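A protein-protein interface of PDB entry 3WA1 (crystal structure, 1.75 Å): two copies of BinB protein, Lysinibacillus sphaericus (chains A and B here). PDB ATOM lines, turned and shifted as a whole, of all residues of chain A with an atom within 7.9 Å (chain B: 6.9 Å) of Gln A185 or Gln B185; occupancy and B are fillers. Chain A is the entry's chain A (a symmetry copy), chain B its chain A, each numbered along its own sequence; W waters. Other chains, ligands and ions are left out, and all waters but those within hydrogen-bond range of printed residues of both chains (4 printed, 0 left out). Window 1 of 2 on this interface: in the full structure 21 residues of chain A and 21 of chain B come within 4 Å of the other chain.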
ATOM      1  N   PRO A   9      14.433  10.393  15.511  1.00  0.00           N
ATOM      2  CA  PRO A   9      14.180  11.572  16.370  1.00  0.00           C
ATOM      3  C   PRO A   9      12.829  12.194  16.005  1.00  0.00           C
ATOM      4  O   PRO A   9      12.253  11.900  14.957  1.00  0.00           O
ATOM      5  CB  PRO A   9      15.338  12.550  16.027  1.00  0.00           C
ATOM      6  CG  PRO A   9      15.847  12.117  14.708  1.00  0.00           C
ATOM      7  CD  PRO A   9      15.559  10.635  14.570  1.00  0.00           C
ATOM      8  N   THR A  10      12.337  13.050  16.880  1.00  0.00           N
ATOM      9  CA  THR A  10      11.084  13.735  16.625  1.00  0.00           C
ATOM     10  C   THR A  10      11.373  15.243  16.500  1.00  0.00           C
ATOM     11  O   THR A  10      12.386  15.798  17.014  1.00  0.00           O
ATOM     12  CB  THR A  10      10.028  13.410  17.714  1.00  0.00           C
ATOM     13  OG1 THR A  10      10.409  14.047  18.931  1.00  0.00           O
ATOM     14  CG2 THR A  10       9.954  11.900  17.983  1.00  0.00           C
ATOM     15  N   SER A  11      10.520  15.898  15.731  1.00  0.00           N
ATOM     16  CA  SER A  11      10.479  17.339  15.734  1.00  0.00           C
ATOM     17  C   SER A  11       9.886  17.772  17.103  1.00  0.00           C
ATOM     18  O   SER A  11       8.926  17.164  17.620  1.00  0.00           O
ATOM     19  CB  SER A  11       9.690  17.844  14.507  1.00  0.00           C
ATOM     20  OG  SER A  11      10.582  17.918  13.386  1.00  0.00           O
ATOM     21  N   LEU A  12      10.546  18.728  17.763  1.00  0.00           N
ATOM     22  CA  LEU A  12       9.902  19.440  18.829  1.00  0.00           C
ATOM     23  C   LEU A  12       8.976  20.520  18.214  1.00  0.00           C
ATOM     24  O   LEU A  12       9.349  21.157  17.219  1.00  0.00           O
ATOM     25  CB  LEU A  12      10.986  20.098  19.721  1.00  0.00           C
ATOM     26  CG  LEU A  12      11.725  19.049  20.589  1.00  0.00           C
ATOM     27  CD1 LEU A  12      12.941  19.743  21.242  1.00  0.00           C
ATOM     28  CD2 LEU A  12      10.777  18.431  21.622  1.00  0.00           C
ATOM     29  N   ALA A 182      11.558  37.786  15.224  1.00  0.00           N
ATOM     30  CA  ALA A 182      12.751  36.891  15.073  1.00  0.00           C
ATOM     31  C   ALA A 182      12.428  35.718  15.959  1.00  0.00           C
ATOM     32  O   ALA A 182      12.080  35.866  17.184  1.00  0.00           O
ATOM     33  CB  ALA A 182      13.983  37.667  15.602  1.00  0.00           C
ATOM     34  N   ILE A 183      12.526  34.506  15.400  1.00  0.00           N
ATOM     35  CA  ILE A 183      12.188  33.357  16.205  1.00  0.00           C
ATOM     36  C   ILE A 183      13.305  32.283  16.012  1.00  0.00           C
ATOM     37  O   ILE A 183      13.694  31.977  14.857  1.00  0.00           O
ATOM     38  CB  ILE A 183      10.875  32.753  15.672  1.00  0.00           C
ATOM     39  CG1 ILE A 183       9.702  33.837  15.635  1.00  0.00           C
ATOM     40  CG2 ILE A 183      10.416  31.530  16.514  1.00  0.00           C
ATOM     41  CD1 ILE A 183       8.377  33.283  15.039  1.00  0.00           C
ATOM     42  N   PRO A 184      13.776  31.692  17.112  1.00  0.00           N
ATOM     43  CA  PRO A 184      14.786  30.621  16.995  1.00  0.00           C
ATOM     44  C   PRO A 184      14.261  29.390  16.321  1.00  0.00           C
ATOM     45  O   PRO A 184      13.108  29.092  16.423  1.00  0.00           O
ATOM     46  CB  PRO A 184      15.070  30.268  18.445  1.00  0.00           C
ATOM     47  CG  PRO A 184      14.549  31.373  19.284  1.00  0.00           C
ATOM     48  CD  PRO A 184      13.373  31.930  18.531  1.00  0.00           C
ATOM     49  N   GLN A 185      15.152  28.625  15.729  1.00  0.00           N
ATOM     50  CA  GLN A 185      14.781  27.292  15.233  1.00  0.00           C
ATOM     51  C   GLN A 185      14.753  26.327  16.422  1.00  0.00           C
ATOM     52  O   GLN A 185      15.617  26.358  17.269  1.00  0.00           O
ATOM     53  CB  GLN A 185      15.889  26.894  14.234  1.00  0.00           C
ATOM     54  CG  GLN A 185      15.796  25.444  13.743  1.00  0.00           C
ATOM     55  CD  GLN A 185      16.892  25.144  12.677  1.00  0.00           C
ATOM     56  OE1 GLN A 185      17.953  25.791  12.658  1.00  0.00           O
ATOM     57  NE2 GLN A 185      16.552  24.368  11.706  1.00  0.00           N
ATOM     58  N   LEU A 186      13.740  25.470  16.448  1.00  0.00           N
ATOM     59  CA  LEU A 186      13.584  24.462  17.493  1.00  0.00           C
ATOM     60  C   LEU A 186      14.496  23.289  17.090  1.00  0.00           C
ATOM     61  O   LEU A 186      14.460  22.923  15.921  1.00  0.00           O
ATOM     62  CB  LEU A 186      12.185  24.004  17.570  1.00  0.00           C
ATOM     63  CG  LEU A 186      11.159  25.044  18.065  1.00  0.00           C
ATOM     64  CD1 LEU A 186       9.727  24.561  17.720  1.00  0.00           C
ATOM     65  CD2 LEU A 186      11.316  25.141  19.597  1.00  0.00           C
ATOM     66  N   PRO A 187      15.279  22.790  18.018  1.00  0.00           N
ATOM     67  CA  PRO A 187      16.206  21.685  17.703  1.00  0.00           C
ATOM     68  C   PRO A 187      15.472  20.360  17.592  1.00  0.00           C
ATOM     69  O   PRO A 187      14.395  20.201  18.116  1.00  0.00           O
ATOM     70  CB  PRO A 187      17.122  21.652  18.944  1.00  0.00           C
ATOM     71  CG  PRO A 187      16.258  22.075  20.037  1.00  0.00           C
ATOM     72  CD  PRO A 187      15.358  23.165  19.452  1.00  0.00           C
ATOM     73  N   GLN A 188      16.072  19.364  16.944  1.00  0.00           N
ATOM     74  CA  GLN A 188      15.392  18.082  16.925  1.00  0.00           C
ATOM     75  C   GLN A 188      15.812  17.309  18.182  1.00  0.00           C
ATOM     76  O   GLN A 188      16.893  17.577  18.658  1.00  0.00           O
ATOM     77  CB  GLN A 188      15.723  17.267  15.649  1.00  0.00           C
ATOM     78  CG  GLN A 188      17.091  16.632  15.514  1.00  0.00           C
ATOM     79  CD  GLN A 188      17.249  15.901  14.166  1.00  0.00           C
ATOM     80  OE1 GLN A 188      16.419  16.078  13.259  1.00  0.00           O
ATOM     81  NE2 GLN A 188      18.368  15.138  14.004  1.00  0.00           N
ATOM     82  N   THR A 189      14.962  16.392  18.636  1.00  0.00           N
ATOM     83  CA  THR A 189      15.277  15.598  19.820  1.00  0.00           C
ATOM     84  C   THR A 189      16.407  14.638  19.544  1.00  0.00           C
ATOM     85  O   THR A 189      16.715  14.312  18.374  1.00  0.00           O
ATOM     86  CB  THR A 189      14.094  14.761  20.248  1.00  0.00           C
ATOM     87  OG1 THR A 189      13.734  13.869  19.167  1.00  0.00           O
ATOM     88  CG2 THR A 189      12.968  15.636  20.654  1.00  0.00           C
ATOM     89  N   VAL A 215      18.928  16.081  23.453  1.00  0.00           N
ATOM     90  CA  VAL A 215      17.860  17.152  23.484  1.00  0.00           C
ATOM     91  C   VAL A 215      16.501  16.556  23.746  1.00  0.00           C
ATOM     92  O   VAL A 215      16.011  15.760  22.934  1.00  0.00           O
ATOM     93  CB  VAL A 215      17.891  17.916  22.111  1.00  0.00           C
ATOM     94  CG1 VAL A 215      16.708  18.923  22.015  1.00  0.00           C
ATOM     95  CG2 VAL A 215      19.240  18.626  21.991  1.00  0.00           C
ATOM     96  N   SER A 218      12.048  21.858  24.301  1.00  0.00           N
ATOM     97  CA  SER A 218      12.433  23.237  23.992  1.00  0.00           C
ATOM     98  C   SER A 218      11.173  24.122  24.050  1.00  0.00           C
ATOM     99  O   SER A 218      10.052  23.671  23.738  1.00  0.00           O
ATOM    100  CB  SER A 218      12.942  23.366  22.561  1.00  0.00           C
ATOM    101  OG  SER A 218      14.319  23.025  22.485  1.00  0.00           O
ATOM    102  N   ALA A 219      11.370  25.391  24.452  1.00  0.00           N
ATOM    103  CA  ALA A 219      10.202  26.336  24.509  1.00  0.00           C
ATOM    104  C   ALA A 219      10.649  27.592  23.883  1.00  0.00           C
ATOM    105  O   ALA A 219      11.866  27.954  23.934  1.00  0.00           O
ATOM    106  CB  ALA A 219       9.731  26.576  25.937  1.00  0.00           C
ATOM    107  N   LEU A 220       9.696  28.345  23.278  1.00  0.00           N
ATOM    108  CA  LEU A 220      10.025  29.708  22.798  1.00  0.00           C
ATOM    109  C   LEU A 220       9.504  30.716  23.820  1.00  0.00           C
ATOM    110  O   LEU A 220       8.325  30.685  24.165  1.00  0.00           O
ATOM    111  CB  LEU A 220       9.289  29.951  21.454  1.00  0.00           C
ATOM    112  CG  LEU A 220       9.690  28.925  20.396  1.00  0.00           C
ATOM    113  CD1 LEU A 220       8.882  29.185  19.127  1.00  0.00           C
ATOM    114  CD2 LEU A 220      11.130  29.113  20.044  1.00  0.00           C
ATOM    115  N   TYR A 242      11.598  36.114  20.393  1.00  0.00           N
ATOM    116  CA  TYR A 242      11.533  34.937  21.279  1.00  0.00           C
ATOM    117  C   TYR A 242      12.952  34.429  21.514  1.00  0.00           C
ATOM    118  O   TYR A 242      13.773  34.469  20.574  1.00  0.00           O
ATOM    119  CB  TYR A 242      10.790  33.780  20.600  1.00  0.00           C
ATOM    120  CG  TYR A 242       9.281  34.050  20.542  1.00  0.00           C
ATOM    121  CD1 TYR A 242       8.757  34.735  19.446  1.00  0.00           C
ATOM    122  CD2 TYR A 242       8.420  33.631  21.560  1.00  0.00           C
ATOM    123  CE1 TYR A 242       7.320  34.971  19.380  1.00  0.00           C
ATOM    124  CE2 TYR A 242       7.021  33.853  21.517  1.00  0.00           C
ATOM    125  CZ  TYR A 242       6.503  34.505  20.386  1.00  0.00           C
ATOM    126  OH  TYR A 242       5.167  34.763  20.184  1.00  0.00           O
ATOM    127  N   LEU A 244      15.228  30.990  22.833  1.00  0.00           N
ATOM    128  CA  LEU A 244      15.025  29.547  22.910  1.00  0.00           C
ATOM    129  C   LEU A 244      15.436  29.074  24.305  1.00  0.00           C
ATOM    130  O   LEU A 244      16.467  29.495  24.773  1.00  0.00           O
ATOM    131  CB  LEU A 244      15.959  28.909  21.872  1.00  0.00           C
ATOM    132  CG  LEU A 244      15.933  27.340  21.950  1.00  0.00           C
ATOM    133  CD1 LEU A 244      14.538  26.800  21.518  1.00  0.00           C
ATOM    134  CD2 LEU A 244      16.975  26.892  20.891  1.00  0.00           C
ATOM    135  N   GLU A 246      16.244  25.504  25.791  1.00  0.00           N
ATOM    136  CA  GLU A 246      16.374  24.050  25.498  1.00  0.00           C
ATOM    137  C   GLU A 246      16.375  23.283  26.806  1.00  0.00           C
ATOM    138  O   GLU A 246      16.959  23.747  27.751  1.00  0.00           O
ATOM    139  CB  GLU A 246      17.728  23.781  24.822  1.00  0.00           C
ATOM    140  CG  GLU A 246      18.033  24.547  23.583  1.00  0.00           C
ATOM    141  CD  GLU A 246      19.388  24.172  23.024  1.00  0.00           C
ATOM    142  OE1 GLU A 246      20.288  23.946  23.840  1.00  0.00           O
ATOM    143  OE2 GLU A 246      19.539  24.207  21.814  1.00  0.00           O
ATOM    144  N   LYS A 354      19.131  30.477  24.798  1.00  0.00           N
ATOM    145  CA  LYS A 354      19.849  30.915  23.616  1.00  0.00           C
ATOM    146  C   LYS A 354      19.160  32.123  22.907  1.00  0.00           C
ATOM    147  O   LYS A 354      17.942  32.150  22.809  1.00  0.00           O
ATOM    148  CB  LYS A 354      19.909  29.736  22.624  1.00  0.00           C
ATOM    149  CG  LYS A 354      20.944  28.664  23.125  1.00  0.00           C
ATOM    150  CD  LYS A 354      21.067  27.587  21.993  1.00  0.00           C
ATOM    151  CE  LYS A 354      22.117  26.600  22.470  1.00  0.00           C
ATOM    152  NZ  LYS A 354      22.199  25.466  21.470  1.00  0.00           N
ATOM    153  N   ARG A 355      19.976  32.955  22.288  1.00  0.00           N
ATOM    154  CA  ARG A 355      19.495  34.004  21.352  1.00  0.00           C
ATOM    155  C   ARG A 355      19.106  33.393  20.026  1.00  0.00           C
ATOM    156  O   ARG A 355      19.500  32.255  19.712  1.00  0.00           O
ATOM    157  CB  ARG A 355      20.589  35.082  21.221  1.00  0.00           C
ATOM    158  CG  ARG A 355      20.830  35.759  22.583  1.00  0.00           C
ATOM    159  CD  ARG A 355      21.603  37.075  22.388  1.00  0.00           C
ATOM    160  NE  ARG A 355      21.896  37.588  23.714  1.00  0.00           N
ATOM    161  CZ  ARG A 355      23.049  37.382  24.356  1.00  0.00           C
ATOM    162  NH1 ARG A 355      24.079  36.801  23.724  1.00  0.00           N
ATOM    163  NH2 ARG A 355      23.192  37.782  25.606  1.00  0.00           N
ATOM    164  N   VAL A 356      18.386  34.175  19.189  1.00  0.00           N
ATOM    165  CA  VAL A 356      18.024  33.721  17.861  1.00  0.00           C
ATOM    166  C   VAL A 356      19.265  33.349  17.049  1.00  0.00           C
ATOM    167  O   VAL A 356      19.217  32.402  16.249  1.00  0.00           O
ATOM    168  CB  VAL A 356      17.144  34.779  17.147  1.00  0.00           C
ATOM    169  CG1 VAL A 356      16.912  34.382  15.664  1.00  0.00           C
ATOM    170  CG2 VAL A 356      15.748  34.769  17.835  1.00  0.00           C
ATOM    171  N   ASN A 357      20.330  34.104  17.257  1.00  0.00           N
ATOM    172  CA  ASN A 357      21.595  33.873  16.507  1.00  0.00           C
ATOM    173  C   ASN A 357      22.374  32.637  17.016  1.00  0.00           C
ATOM    174  O   ASN A 357      23.490  32.378  16.491  1.00  0.00           O
ATOM    175  CB  ASN A 357      22.493  35.110  16.499  1.00  0.00           C
ATOM    176  CG  ASN A 357      22.987  35.509  17.868  1.00  0.00           C
ATOM    177  OD1 ASN A 357      22.931  34.748  18.833  1.00  0.00           O
ATOM    178  ND2 ASN A 357      23.471  36.767  17.980  1.00  0.00           N
ATOM    179  N   GLY A 358      21.803  31.891  17.970  1.00  0.00           N
ATOM    180  CA  GLY A 358      22.494  30.719  18.484  1.00  0.00           C
ATOM    181  C   GLY A 358      23.420  30.970  19.677  1.00  0.00           C
ATOM    182  O   GLY A 358      23.872  29.993  20.292  1.00  0.00           O
ATOM    183  N   SER B  11      14.983  28.655   5.205  1.00  0.00           N
ATOM    184  CA  SER B  11      15.346  27.274   5.413  1.00  0.00           C
ATOM    185  C   SER B  11      16.465  26.942   4.388  1.00  0.00           C
ATOM    186  O   SER B  11      16.418  27.358   3.212  1.00  0.00           O
ATOM    187  CB  SER B  11      14.092  26.381   5.302  1.00  0.00           C
ATOM    188  OG  SER B  11      13.435  26.352   6.577  1.00  0.00           O
ATOM    189  N   ILE B 183      20.256  11.432  10.301  1.00  0.00           N
ATOM    190  CA  ILE B 183      20.553  12.573   9.469  1.00  0.00           C
ATOM    191  C   ILE B 183      20.510  13.852  10.365  1.00  0.00           C
ATOM    192  O   ILE B 183      19.539  14.047  11.140  1.00  0.00           O
ATOM    193  CB  ILE B 183      19.440  12.715   8.414  1.00  0.00           C
ATOM    194  CG1 ILE B 183      19.260  11.373   7.565  1.00  0.00           C
ATOM    195  CG2 ILE B 183      19.707  13.902   7.446  1.00  0.00           C
ATOM    196  CD1 ILE B 183      18.099  11.455   6.534  1.00  0.00           C
ATOM    197  N   PRO B 184      21.512  14.722  10.229  1.00  0.00           N
ATOM    198  CA  PRO B 184      21.497  15.983  10.999  1.00  0.00           C
ATOM    199  C   PRO B 184      20.383  16.902  10.599  1.00  0.00           C
ATOM    200  O   PRO B 184      19.976  16.903   9.476  1.00  0.00           O
ATOM    201  CB  PRO B 184      22.805  16.640  10.590  1.00  0.00           C
ATOM    202  CG  PRO B 184      23.652  15.596   9.965  1.00  0.00           C
ATOM    203  CD  PRO B 184      22.694  14.633   9.321  1.00  0.00           C
ATOM    204  N   GLN B 185      19.981  17.760  11.511  1.00  0.00           N
ATOM    205  CA  GLN B 185      19.055  18.847  11.158  1.00  0.00           C
ATOM    206  C   GLN B 185      19.857  19.958  10.476  1.00  0.00           C
ATOM    207  O   GLN B 185      20.938  20.298  10.902  1.00  0.00           O
ATOM    208  CB  GLN B 185      18.464  19.343  12.496  1.00  0.00           C
ATOM    209  CG  GLN B 185      17.614  20.613  12.369  1.00  0.00           C
ATOM    210  CD  GLN B 185      16.984  21.002  13.741  1.00  0.00           C
ATOM    211  OE1 GLN B 185      17.523  20.660  14.807  1.00  0.00           O
ATOM    212  NE2 GLN B 185      15.791  21.486  13.707  1.00  0.00           N
ATOM    213  N   LEU B 186      19.288  20.515   9.414  1.00  0.00           N
ATOM    214  CA  LEU B 186      19.902  21.610   8.669  1.00  0.00           C
ATOM    215  C   LEU B 186      19.572  22.893   9.452  1.00  0.00           C
ATOM    216  O   LEU B 186      18.418  23.033   9.842  1.00  0.00           O
ATOM    217  CB  LEU B 186      19.341  21.695   7.309  1.00  0.00           C
ATOM    218  CG  LEU B 186      19.680  20.524   6.364  1.00  0.00           C
ATOM    219  CD1 LEU B 186      18.723  20.552   5.144  1.00  0.00           C
ATOM    220  CD2 LEU B 186      21.132  20.734   5.885  1.00  0.00           C
ATOM    221  N   PRO B 187      20.557  23.729   9.682  1.00  0.00           N
ATOM    222  CA  PRO B 187      20.327  24.967  10.454  1.00  0.00           C
ATOM    223  C   PRO B 187      19.616  26.016   9.618  1.00  0.00           C
ATOM    224  O   PRO B 187      19.649  25.977   8.412  1.00  0.00           O
ATOM    225  CB  PRO B 187      21.762  25.447  10.753  1.00  0.00           C
ATOM    226  CG  PRO B 187      22.534  25.007   9.598  1.00  0.00           C
ATOM    227  CD  PRO B 187      21.965  23.637   9.222  1.00  0.00           C
ATOM    228  N   GLN B 188      18.997  27.009  10.255  1.00  0.00           N
ATOM    229  CA  GLN B 188      18.398  28.048   9.436  1.00  0.00           C
ATOM    230  C   GLN B 188      19.474  29.106   9.159  1.00  0.00           C
ATOM    231  O   GLN B 188      20.364  29.212   9.973  1.00  0.00           O
ATOM    232  CB  GLN B 188      17.167  28.692  10.122  1.00  0.00           C
ATOM    233  CG  GLN B 188      17.381  29.627  11.294  1.00  0.00           C
ATOM    234  CD  GLN B 188      16.044  30.134  11.870  1.00  0.00           C
ATOM    235  OE1 GLN B 188      14.975  29.596  11.534  1.00  0.00           O
ATOM    236  NE2 GLN B 188      16.110  31.123  12.807  1.00  0.00           N
ATOM    237  N   THR B 189      19.332  29.833   8.055  1.00  0.00           N
ATOM    238  CA  THR B 189      20.298  30.871   7.710  1.00  0.00           C
ATOM    239  C   THR B 189      20.215  32.030   8.672  1.00  0.00           C
ATOM    240  O   THR B 189      19.197  32.222   9.376  1.00  0.00           O
ATOM    241  CB  THR B 189      20.031  31.433   6.333  1.00  0.00           C
ATOM    242  OG1 THR B 189      18.702  32.003   6.308  1.00  0.00           O
ATOM    243  CG2 THR B 189      20.210  30.377   5.307  1.00  0.00           C
ATOM    244  N   SER B 218      24.751  24.844   4.030  1.00  0.00           N
ATOM    245  CA  SER B 218      24.973  23.581   4.737  1.00  0.00           C
ATOM    246  C   SER B 218      24.795  22.422   3.737  1.00  0.00           C
ATOM    247  O   SER B 218      23.989  22.507   2.788  1.00  0.00           O
ATOM    248  CB  SER B 218      23.914  23.347   5.807  1.00  0.00           C
ATOM    249  OG  SER B 218      24.260  24.016   7.012  1.00  0.00           O
ATOM    250  N   LEU B 220      24.662  17.893   3.455  1.00  0.00           N
ATOM    251  CA  LEU B 220      24.707  16.601   4.180  1.00  0.00           C
ATOM    252  C   LEU B 220      25.693  15.681   3.462  1.00  0.00           C
ATOM    253  O   LEU B 220      25.563  15.464   2.259  1.00  0.00           O
ATOM    254  CB  LEU B 220      23.300  15.950   4.121  1.00  0.00           C
ATOM    255  CG  LEU B 220      22.235  16.849   4.744  1.00  0.00           C
ATOM    256  CD1 LEU B 220      20.873  16.176   4.592  1.00  0.00           C
ATOM    257  CD2 LEU B 220      22.495  16.985   6.209  1.00  0.00           C
ATOM    258  N   LEU B 244      26.973  16.740   9.035  1.00  0.00           N
ATOM    259  CA  LEU B 244      26.593  18.072   8.575  1.00  0.00           C
ATOM    260  C   LEU B 244      27.867  18.866   8.285  1.00  0.00           C
ATOM    261  O   LEU B 244      28.772  18.814   9.083  1.00  0.00           O
ATOM    262  CB  LEU B 244      25.840  18.745   9.733  1.00  0.00           C
ATOM    263  CG  LEU B 244      25.493  20.243   9.410  1.00  0.00           C
ATOM    264  CD1 LEU B 244      24.457  20.320   8.251  1.00  0.00           C
ATOM    265  CD2 LEU B 244      24.811  20.760  10.705  1.00  0.00           C
ATOM    266  N   GLU B 246      28.563  22.722   7.783  1.00  0.00           N
ATOM    267  CA  GLU B 246      27.971  24.088   7.773  1.00  0.00           C
ATOM    268  C   GLU B 246      28.941  25.040   7.101  1.00  0.00           C
ATOM    269  O   GLU B 246      30.120  24.911   7.310  1.00  0.00           O
ATOM    270  CB  GLU B 246      27.791  24.581   9.218  1.00  0.00           C
ATOM    271  CG  GLU B 246      26.994  23.721  10.134  1.00  0.00           C
ATOM    272  CD  GLU B 246      26.892  24.335  11.514  1.00  0.00           C
ATOM    273  OE1 GLU B 246      27.892  24.922  11.942  1.00  0.00           O
ATOM    274  OE2 GLU B 246      25.875  24.134  12.156  1.00  0.00           O
ATOM    275  N   VAL B 356      25.698  13.914  13.910  1.00  0.00           N
ATOM    276  CA  VAL B 356      24.260  14.025  14.060  1.00  0.00           C
ATOM    277  C   VAL B 356      23.891  14.563  15.443  1.00  0.00           C
ATOM    278  O   VAL B 356      22.913  15.314  15.572  1.00  0.00           O
ATOM    279  CB  VAL B 356      23.575  12.670  13.750  1.00  0.00           C
ATOM    280  CG1 VAL B 356      22.061  12.734  14.091  1.00  0.00           C
ATOM    281  CG2 VAL B 356      23.677  12.433  12.216  1.00  0.00           C
HETATM  282  O   HOH W   1      12.947  20.831  14.682  1.00  0.00           O
HETATM  283  O   HOH W   2      16.214  24.418   8.649  1.00  0.00           O
HETATM  284  O   HOH W   3      16.579  13.554  11.340  1.00  0.00           O
HETATM  285  O   HOH W   4      12.663  31.710  12.044  1.00  0.00           O
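Ile A183 touches Gln B188, and with the chains exchanged Gln A188 touches Ile B183.
Gln B185 touches its own counterpart, Gln A185.
Gln A185 touches Leu B186, and with the chains exchanged Leu A186 touches Gln B185.
Gln A185 touches Pro B187, and with the chains exchanged Pro A187 touches Gln B185.
13 positions are printed for both chains.
Of the 9 pairs that touch across the chains among the printed residues, 9 have their exchanged pair printed and touching as well.
The backbone carbonyl oxygen (O) of Ile B183 is in hydrogen-bond range of the side-chain amide nitrogen (NE2) of Gln A188.
NE2 of Gln B185 lies within hydrogen-bond range of O of Leu A186, 3.0 Å away.
The side-chain amide oxygen (OE1) of Gln B185 sits at hydrogen-bond distance from the backbone NH (N) of Gln A188, at 2.9 Å.
The backbone carbonyl oxygen (O) of Leu B186 lies within hydrogen-bond range of the side-chain amide nitrogen (NE2) of Gln A185, at 3.0 Å.
The side-chain amide nitrogen (NE2) of Gln B188 sits at hydrogen-bond distance from the backbone carbonyl oxygen (O) of Ile A183, at 3.3 Å.
The backbone NH (N) of Gln B188 sits at hydrogen-bond distance from the side-chain amide oxygen (OE1) of Gln A185, 2.9 Å away.
Gln A185 touches Gln B185.
Gln A185 touches Pro B187 (OE1 to CA, 3.3 Å).
Pro A187 touches Gln B185.
Printed residues of chain A that touch a printed residue of chain B: Ile A183, Gln A185, Leu A186, Pro A187 and Gln A188.
Among the printed residues, 9 pairs touch across the chains.
Water W1 bridges the backbone carbonyl oxygen of Leu A186 (2.9 Å) and the side-chain amide nitrogen of Gln B185 (3.1 Å).
Water W2 lies within hydrogen-bond range of O of Leu B186 (2.9 Å) and NE2 of Gln A185 (3.1 Å).
Water W3 bridges O of Ile B183 and OE1 of Gln A188.
Water W4 bridges the backbone carbonyl oxygen (O) of Ile A183 (3.0 Å) and the side-chain amide oxygen (OE1) of Gln B188 (3.2 Å).
Of chain B, only Gln B185 (3.6 Å), Leu B186 (3.0 Å), Pro B187 (3.3 Å) and Gln B188 (2.9 Å) come within 4 Å of Gln A185.
Of the printed residues of chain A, Gln B188 touches Ile A183 and Gln A185.
Printed residues of chain A within 4 Å of Leu B186: Gln A185 (3.0 Å).
Printed residues of chain B within 4 Å of Pro A187: Gln B185 (3.3 Å).
Ala A182 touches none of the printed residues of chain B.
The nearest residue of chain A that does not touch Gln B185 is Thr A189 (6.3 Å).
The nearest printed residue of chain A that does not touch Pro B187 is Leu A186 (8.3 Å).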
